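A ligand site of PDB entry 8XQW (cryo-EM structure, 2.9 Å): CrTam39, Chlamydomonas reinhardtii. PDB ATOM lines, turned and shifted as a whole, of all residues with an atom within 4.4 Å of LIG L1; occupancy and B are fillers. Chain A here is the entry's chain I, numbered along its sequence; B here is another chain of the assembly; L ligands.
The backbone carbonyl oxygen of Asp 213 lies within hydrogen-bond range of an oxygen (O3) of LG2 L2 (3.0 Å).
An oxygen (O2) of LG2 L2 sits at hydrogen-bond distance from the side-chain carboxylate of Asp 213.
O6 of LIG L1 lies within hydrogen-bond range of NE1 of Trp 218.
NH1 of Arg 200 lies within salt-bridge range of O12 of LIG L1, 2.8 Å away.
The side-chain carboxylate of Asp 213 sits at hydrogen-bond distance from an oxygen (O7) of LIG L1 (3.0 Å).
NH1 of Arg 468 of chain B lies within hydrogen-bond range of O of Trp 211 (3.1 Å).
OD2 of Asp 213 lies within salt-bridge range of NH2 of Arg 468 of chain B (3.7 Å).
The backbone carbonyl oxygen (O) of Trp 206 sits at hydrogen-bond distance from the indole nitrogen (NE1) of Trp 211 (3.2 Å).
Trp 198 touches LIG L1 (N to C7, 3.6 Å).
Trp 206 touches LIG L1.
Trp 211 touches LIG L1.
Leu 221 touches LIG L1.
Gly 251 touches LIG L1.
Ala 255 touches LIG L1 (CB to C27, 3.9 Å).
Arg 468 of chain B touches LIG L1.
Hydrophobic or aromatic side chains within 4 Å of LIG L1: Trp 206, Trp 211, Trp 218, Leu 221 and Ala 255.
Within 4 Å of LIG L1: Trp 198, Arg 200, Trp 206, Trp 211, Asp 213, Trp 218, Leu 221, Gly 251, Ala 255 and Arg 468 of chain B.
Along chain A the residues within 4 Å of LIG L1 span positions 198 to 255.
The nearest printed residue that does not touch LIG L1 is Ala 225 (4.1 Å).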
ATOM      1  N   TRP A 198      15.501  -7.989 -11.229  1.00  0.00           N
ATOM      2  CA  TRP A 198      16.453  -8.820 -11.951  1.00  0.00           C
ATOM      3  C   TRP A 198      15.739  -9.756 -12.922  1.00  0.00           C
ATOM      4  O   TRP A 198      14.570  -9.554 -13.229  1.00  0.00           O
ATOM      5  CB  TRP A 198      17.309  -9.639 -10.989  1.00  0.00           C
ATOM      6  CG  TRP A 198      16.556 -10.632 -10.178  1.00  0.00           C
ATOM      7  CD1 TRP A 198      15.213 -10.678  -9.990  1.00  0.00           C
ATOM      8  CD2 TRP A 198      17.088 -11.757  -9.473  1.00  0.00           C
ATOM      9  NE1 TRP A 198      14.877 -11.749  -9.198  1.00  0.00           N
ATOM     10  CE2 TRP A 198      16.014 -12.424  -8.876  1.00  0.00           C
ATOM     11  CE3 TRP A 198      18.385 -12.254  -9.291  1.00  0.00           C
ATOM     12  CZ2 TRP A 198      16.186 -13.565  -8.090  1.00  0.00           C
ATOM     13  CZ3 TRP A 198      18.551 -13.386  -8.525  1.00  0.00           C
ATOM     14  CH2 TRP A 198      17.457 -14.029  -7.936  1.00  0.00           C
ATOM     15  N   ARG A 200      14.732 -13.746 -14.253  1.00  0.00           N
ATOM     16  CA  ARG A 200      14.429 -15.095 -13.802  1.00  0.00           C
ATOM     17  C   ARG A 200      13.932 -15.891 -15.004  1.00  0.00           C
ATOM     18  O   ARG A 200      12.763 -15.813 -15.360  1.00  0.00           O
ATOM     19  CB  ARG A 200      13.397 -15.087 -12.686  1.00  0.00           C
ATOM     20  CG  ARG A 200      13.987 -14.869 -11.321  1.00  0.00           C
ATOM     21  CD  ARG A 200      12.929 -15.054 -10.252  1.00  0.00           C
ATOM     22  NE  ARG A 200      12.922 -13.938  -9.325  1.00  0.00           N
ATOM     23  CZ  ARG A 200      12.063 -13.797  -8.333  1.00  0.00           C
ATOM     24  NH1 ARG A 200      12.132 -12.750  -7.542  1.00  0.00           N
ATOM     25  NH2 ARG A 200      11.133 -14.726  -8.130  1.00  0.00           N
ATOM     26  N   TRP A 206       7.429 -12.679 -12.894  1.00  0.00           N
ATOM     27  CA  TRP A 206       7.136 -12.813 -11.488  1.00  0.00           C
ATOM     28  C   TRP A 206       6.614 -11.525 -10.863  1.00  0.00           C
ATOM     29  O   TRP A 206       5.804 -11.600  -9.930  1.00  0.00           O
ATOM     30  CB  TRP A 206       8.362 -13.313 -10.720  1.00  0.00           C
ATOM     31  CG  TRP A 206       9.528 -12.411 -10.760  1.00  0.00           C
ATOM     32  CD1 TRP A 206      10.526 -12.423 -11.679  1.00  0.00           C
ATOM     33  CD2 TRP A 206       9.828 -11.352  -9.853  1.00  0.00           C
ATOM     34  NE1 TRP A 206      11.435 -11.446 -11.406  1.00  0.00           N
ATOM     35  CE2 TRP A 206      11.024 -10.770 -10.282  1.00  0.00           C
ATOM     36  CE3 TRP A 206       9.198 -10.846  -8.720  1.00  0.00           C
ATOM     37  CZ2 TRP A 206      11.599  -9.696  -9.634  1.00  0.00           C
ATOM     38  CZ3 TRP A 206       9.769  -9.780  -8.074  1.00  0.00           C
ATOM     39  CH2 TRP A 206      10.957  -9.226  -8.518  1.00  0.00           C
ATOM     40  N   TRP A 211       1.219 -11.491  -4.878  1.00  0.00           N
ATOM     41  CA  TRP A 211       2.002 -11.878  -3.723  1.00  0.00           C
ATOM     42  C   TRP A 211       1.328 -11.529  -2.407  1.00  0.00           C
ATOM     43  O   TRP A 211       1.805 -11.973  -1.359  1.00  0.00           O
ATOM     44  CB  TRP A 211       3.367 -11.204  -3.758  1.00  0.00           C
ATOM     45  CG  TRP A 211       4.215 -11.639  -4.877  1.00  0.00           C
ATOM     46  CD1 TRP A 211       4.593 -10.893  -5.943  1.00  0.00           C
ATOM     47  CD2 TRP A 211       4.815 -12.911  -5.041  1.00  0.00           C
ATOM     48  NE1 TRP A 211       5.383 -11.621  -6.777  1.00  0.00           N
ATOM     49  CE2 TRP A 211       5.541 -12.881  -6.237  1.00  0.00           C
ATOM     50  CE3 TRP A 211       4.802 -14.087  -4.289  1.00  0.00           C
ATOM     51  CZ2 TRP A 211       6.252 -13.974  -6.703  1.00  0.00           C
ATOM     52  CZ3 TRP A 211       5.511 -15.166  -4.759  1.00  0.00           C
ATOM     53  CH2 TRP A 211       6.224 -15.098  -5.945  1.00  0.00           C
ATOM     54  N   ASP A 213       0.421  -8.166  -1.326  1.00  0.00           N
ATOM     55  CA  ASP A 213       0.581  -6.808  -0.859  1.00  0.00           C
ATOM     56  C   ASP A 213       0.084  -5.822  -1.910  1.00  0.00           C
ATOM     57  O   ASP A 213      -0.519  -6.195  -2.908  1.00  0.00           O
ATOM     58  CB  ASP A 213       2.039  -6.518  -0.523  1.00  0.00           C
ATOM     59  CG  ASP A 213       2.958  -6.980  -1.589  1.00  0.00           C
ATOM     60  OD1 ASP A 213       2.454  -7.530  -2.584  1.00  0.00           O
ATOM     61  OD2 ASP A 213       4.186  -6.796  -1.446  1.00  0.00           O
ATOM     62  N   TRP A 218       6.884  -0.856  -2.141  1.00  0.00           N
ATOM     63  CA  TRP A 218       8.300  -0.571  -1.997  1.00  0.00           C
ATOM     64  C   TRP A 218       8.626   0.849  -2.414  1.00  0.00           C
ATOM     65  O   TRP A 218       9.571   1.443  -1.910  1.00  0.00           O
ATOM     66  CB  TRP A 218       9.124  -1.551  -2.819  1.00  0.00           C
ATOM     67  CG  TRP A 218       9.199  -2.894  -2.245  1.00  0.00           C
ATOM     68  CD1 TRP A 218       8.722  -4.037  -2.788  1.00  0.00           C
ATOM     69  CD2 TRP A 218       9.782  -3.263  -1.000  1.00  0.00           C
ATOM     70  NE1 TRP A 218       8.973  -5.089  -1.962  1.00  0.00           N
ATOM     71  CE2 TRP A 218       9.622  -4.644  -0.856  1.00  0.00           C
ATOM     72  CE3 TRP A 218      10.429  -2.551   0.026  1.00  0.00           C
ATOM     73  CZ2 TRP A 218      10.087  -5.331   0.256  1.00  0.00           C
ATOM     74  CZ3 TRP A 218      10.877  -3.234   1.111  1.00  0.00           C
ATOM     75  CH2 TRP A 218      10.705  -4.601   1.228  1.00  0.00           C
ATOM     76  N   LEU A 221       8.124   3.066   0.730  1.00  0.00           N
ATOM     77  CA  LEU A 221       9.227   3.030   1.670  1.00  0.00           C
ATOM     78  C   LEU A 221      10.475   3.693   1.102  1.00  0.00           C
ATOM     79  O   LEU A 221      11.194   4.386   1.823  1.00  0.00           O
ATOM     80  CB  LEU A 221       9.532   1.589   2.057  1.00  0.00           C
ATOM     81  CG  LEU A 221       8.384   0.771   2.626  1.00  0.00           C
ATOM     82  CD1 LEU A 221       8.816  -0.652   2.763  1.00  0.00           C
ATOM     83  CD2 LEU A 221       7.984   1.302   3.952  1.00  0.00           C
ATOM     84  N   ALA A 222      10.744   3.494  -0.184  1.00  0.00           N
ATOM     85  CA  ALA A 222      11.861   4.195  -0.815  1.00  0.00           C
ATOM     86  C   ALA A 222      11.695   5.701  -0.699  1.00  0.00           C
ATOM     87  O   ALA A 222      12.649   6.403  -0.348  1.00  0.00           O
ATOM     88  CB  ALA A 222      11.973   3.791  -2.284  1.00  0.00           C
ATOM     89  N   ALA A 225      12.372   6.860   2.859  1.00  0.00           N
ATOM     90  CA  ALA A 225      13.794   6.914   3.159  1.00  0.00           C
ATOM     91  C   ALA A 225      14.444   8.130   2.519  1.00  0.00           C
ATOM     92  O   ALA A 225      15.251   8.813   3.157  1.00  0.00           O
ATOM     93  CB  ALA A 225      14.481   5.639   2.686  1.00  0.00           C
ATOM     94  N   ALA A 228      13.454  11.329   4.449  1.00  0.00           N
ATOM     95  CA  ALA A 228      14.120  11.458   5.746  1.00  0.00           C
ATOM     96  C   ALA A 228      15.594  11.811   5.586  1.00  0.00           C
ATOM     97  O   ALA A 228      16.093  12.740   6.231  1.00  0.00           O
ATOM     98  CB  ALA A 228      13.970  10.164   6.545  1.00  0.00           C
ATOM     99  N   LEU A 248      11.354  14.336   8.341  1.00  0.00           N
ATOM    100  CA  LEU A 248      11.208  13.205   9.251  1.00  0.00           C
ATOM    101  C   LEU A 248       9.759  12.951   9.629  1.00  0.00           C
ATOM    102  O   LEU A 248       9.372  11.806   9.835  1.00  0.00           O
ATOM    103  CB  LEU A 248      12.063  13.415  10.499  1.00  0.00           C
ATOM    104  CG  LEU A 248      13.468  12.819  10.390  1.00  0.00           C
ATOM    105  CD1 LEU A 248      14.329  13.327  11.508  1.00  0.00           C
ATOM    106  CD2 LEU A 248      13.390  11.320  10.435  1.00  0.00           C
ATOM    107  N   GLY A 251       8.568  11.095   6.673  1.00  0.00           N
ATOM    108  CA  GLY A 251       9.167   9.777   6.671  1.00  0.00           C
ATOM    109  C   GLY A 251       8.493   8.829   7.635  1.00  0.00           C
ATOM    110  O   GLY A 251       8.247   7.672   7.303  1.00  0.00           O
ATOM    111  N   ALA A 255       6.492   5.575   6.330  1.00  0.00           N
ATOM    112  CA  ALA A 255       6.907   4.244   6.742  1.00  0.00           C
ATOM    113  C   ALA A 255       5.768   3.492   7.388  1.00  0.00           C
ATOM    114  O   ALA A 255       5.606   2.286   7.162  1.00  0.00           O
ATOM    115  CB  ALA A 255       8.088   4.336   7.703  1.00  0.00           C
ATOM    116  N   ARG B 468       2.865  -9.764   7.119  1.00  0.00           N
ATOM    117  CA  ARG B 468       2.549 -11.108   6.676  1.00  0.00           C
ATOM    118  C   ARG B 468       3.270 -12.172   7.480  1.00  0.00           C
ATOM    119  O   ARG B 468       3.180 -13.343   7.125  1.00  0.00           O
ATOM    120  CB  ARG B 468       2.892 -11.267   5.196  1.00  0.00           C
ATOM    121  CG  ARG B 468       1.729 -10.930   4.281  1.00  0.00           C
ATOM    122  CD  ARG B 468       2.140 -10.901   2.832  1.00  0.00           C
ATOM    123  NE  ARG B 468       3.189  -9.929   2.591  1.00  0.00           N
ATOM    124  CZ  ARG B 468       3.994  -9.968   1.538  1.00  0.00           C
ATOM    125  NH1 ARG B 468       3.871 -10.937   0.651  1.00  0.00           N
ATOM    126  NH2 ARG B 468       4.940  -9.052   1.391  1.00  0.00           N
HETATM  127  O1  LIG L   1      10.349  -8.264  -4.175  1.00  0.00           O
HETATM  128  C1  LIG L   1      11.654  -8.752  -3.961  1.00  0.00           C
HETATM  129  C2  LIG L   1      12.655  -7.642  -4.157  1.00  0.00           C
HETATM  130  C3  LIG L   1      12.811  -6.875  -2.856  1.00  0.00           C
HETATM  131  O2  LIG L   1      13.894  -8.148  -4.617  1.00  0.00           O
HETATM  132  C4  LIG L   1      14.039  -8.544  -5.966  1.00  0.00           C
HETATM  133  O3  LIG L   1      13.482  -9.566  -6.343  1.00  0.00           O
HETATM  134  C5  LIG L   1      15.278  -8.088  -6.723  1.00  0.00           C
HETATM  135  C6  LIG L   1      15.213  -6.576  -6.890  1.00  0.00           C
HETATM  136  C7  LIG L   1      14.468  -6.273  -8.186  1.00  0.00           C
HETATM  137  C8  LIG L   1      14.410  -4.754  -8.388  1.00  0.00           C
HETATM  138  C9  LIG L   1      15.738  -4.117  -8.066  1.00  0.00           C
HETATM  139  C10 LIG L   1      15.511  -2.692  -7.555  1.00  0.00           C
HETATM  140  C11 LIG L   1      16.315  -2.466  -6.274  1.00  0.00           C
HETATM  141  C12 LIG L   1      17.013  -1.117  -6.325  1.00  0.00           C
HETATM  142  C13 LIG L   1      17.901  -1.034  -7.549  1.00  0.00           C
HETATM  143  C14 LIG L   1      18.863   0.146  -7.432  1.00  0.00           C
HETATM  144  O4  LIG L   1      12.803  -5.493  -3.155  1.00  0.00           O
HETATM  145  C15 LIG L   1      13.738  -4.661  -2.496  1.00  0.00           C
HETATM  146  O5  LIG L   1      14.482  -5.164  -1.675  1.00  0.00           O
HETATM  147  C16 LIG L   1      13.598  -3.153  -2.556  1.00  0.00           C
HETATM  148  C17 LIG L   1      13.862  -2.583  -1.162  1.00  0.00           C
HETATM  149  C18 LIG L   1      13.788  -1.058  -1.194  1.00  0.00           C
HETATM  150  C19 LIG L   1      13.627  -0.552   0.245  1.00  0.00           C
HETATM  151  C20 LIG L   1      14.231   0.849   0.383  1.00  0.00           C
HETATM  152  C21 LIG L   1      14.428   1.187   1.859  1.00  0.00           C
HETATM  153  C22 LIG L   1      13.111   0.937   2.599  1.00  0.00           C
HETATM  154  C23 LIG L   1      13.340   0.800   4.104  1.00  0.00           C
HETATM  155  C24 LIG L   1      13.740   2.148   4.710  1.00  0.00           C
HETATM  156  C25 LIG L   1      12.563   2.697   5.520  1.00  0.00           C
HETATM  157  C26 LIG L   1      13.095   3.816   6.416  1.00  0.00           C
HETATM  158  C27 LIG L   1      11.955   4.623   6.982  1.00  0.00           C
HETATM  159  C28 LIG L   1      12.504   5.894   7.553  1.00  0.00           C
HETATM  160  C29 LIG L   1      11.592   6.387   8.621  1.00  0.00           C
HETATM  161  C30 LIG L   1      12.240   7.526   9.362  1.00  0.00           C
HETATM  162  C31 LIG L   1       9.348  -9.033  -3.554  1.00  0.00           C
HETATM  163  C32 LIG L   1       7.952  -8.526  -3.676  1.00  0.00           C
HETATM  164  O6  LIG L   1       7.902  -7.197  -3.343  1.00  0.00           O
HETATM  165  C33 LIG L   1       7.203  -9.283  -2.645  1.00  0.00           C
HETATM  166  O7  LIG L   1       5.875  -8.929  -2.714  1.00  0.00           O
HETATM  167  C34 LIG L   1       7.325 -10.762  -2.777  1.00  0.00           C
HETATM  168  O8  LIG L   1       7.094 -11.308  -1.536  1.00  0.00           O
HETATM  169  C35 LIG L   1       8.665 -11.243  -3.221  1.00  0.00           C
HETATM  170  C36 LIG L   1       8.499 -12.491  -4.024  1.00  0.00           C
HETATM  171  O9  LIG L   1       9.372 -10.334  -4.019  1.00  0.00           O
HETATM  172  S1  LIG L   1      10.087 -13.272  -4.175  1.00  0.00           S
HETATM  173  O10 LIG L   1      11.157 -12.371  -3.834  1.00  0.00           O
HETATM  174  O11 LIG L   1      10.133 -14.477  -3.343  1.00  0.00           O
HETATM  175  O12 LIG L   1      10.404 -13.566  -5.539  1.00  0.00           O
HETATM  176  C1  LG2 L   2       3.446  -6.830  -7.158  1.00  0.00           C
HETATM  177  O1  LG2 L   2       4.462  -5.868  -6.977  1.00  0.00           O
HETATM  178  C2  LG2 L   2       2.669  -6.858  -5.874  1.00  0.00           C
HETATM  179  O2  LG2 L   2       3.592  -7.276  -4.939  1.00  0.00           O
HETATM  180  C3  LG2 L   2       1.666  -7.975  -6.061  1.00  0.00           C
HETATM  181  O3  LG2 L   2       0.861  -7.887  -4.936  1.00  0.00           O
HETATM  182  C4  LG2 L   2       0.778  -7.721  -7.298  1.00  0.00           C
HETATM  183  O4  LG2 L   2      -0.154  -6.778  -6.971  1.00  0.00           O
HETATM  184  C5  LG2 L   2       1.636  -7.195  -8.480  1.00  0.00           C
HETATM  185  O5  LG2 L   2      -0.497  -7.199  -9.403  1.00  0.00           O
HETATM  186  C6  LG2 L   2       0.704  -6.510  -9.487  1.00  0.00           C
HETATM  187  O6  LG2 L   2       2.591  -6.252  -8.084  1.00  0.00           O
HETATM  188  C7  LG2 L   2       4.607  -4.980  -8.049  1.00  0.00           C
HETATM  189  C8  LG2 L   2       6.109  -4.867  -8.349  1.00  0.00           C
HETATM  190  C9  LG2 L   2       6.344  -3.506  -8.967  1.00  0.00           C
HETATM  191  O7  LG2 L   2       6.798  -4.817  -7.140  1.00  0.00           O
HETATM  192  C10 LG2 L   2       8.107  -5.172  -7.153  1.00  0.00           C
HETATM  193  O8  LG2 L   2       8.383  -6.361  -7.077  1.00  0.00           O
HETATM  194  C11 LG2 L   2       9.018  -4.035  -6.836  1.00  0.00           C
HETATM  195  C12 LG2 L   2      10.433  -4.504  -6.638  1.00  0.00           C
HETATM  196  C13 LG2 L   2      11.434  -3.373  -6.784  1.00  0.00           C
HETATM  197  C14 LG2 L   2      11.006  -2.265  -5.856  1.00  0.00           C
HETATM  198  C15 LG2 L   2      11.576  -0.956  -6.353  1.00  0.00           C
HETATM  199  C16 LG2 L   2      12.337  -0.293  -5.236  1.00  0.00           C
HETATM  200  C17 LG2 L   2      12.569   1.133  -5.667  1.00  0.00           C
HETATM  201  O9  LG2 L   2       7.517  -3.609  -9.711  1.00  0.00           O
HETATM  202  C18 LG2 L   2       8.048  -2.455 -10.127  1.00  0.00           C
HETATM  203  O10 LG2 L   2       7.819  -1.440  -9.465  1.00  0.00           O
HETATM  204  C19 LG2 L   2       8.481  -2.454 -11.554  1.00  0.00           C
HETATM  205  C20 LG2 L   2       9.953  -2.770 -11.672  1.00  0.00           C
HETATM  206  C21 LG2 L   2      10.733  -1.480 -11.658  1.00  0.00           C
HETATM  207  C22 LG2 L   2      10.513  -0.782 -13.000  1.00  0.00           C
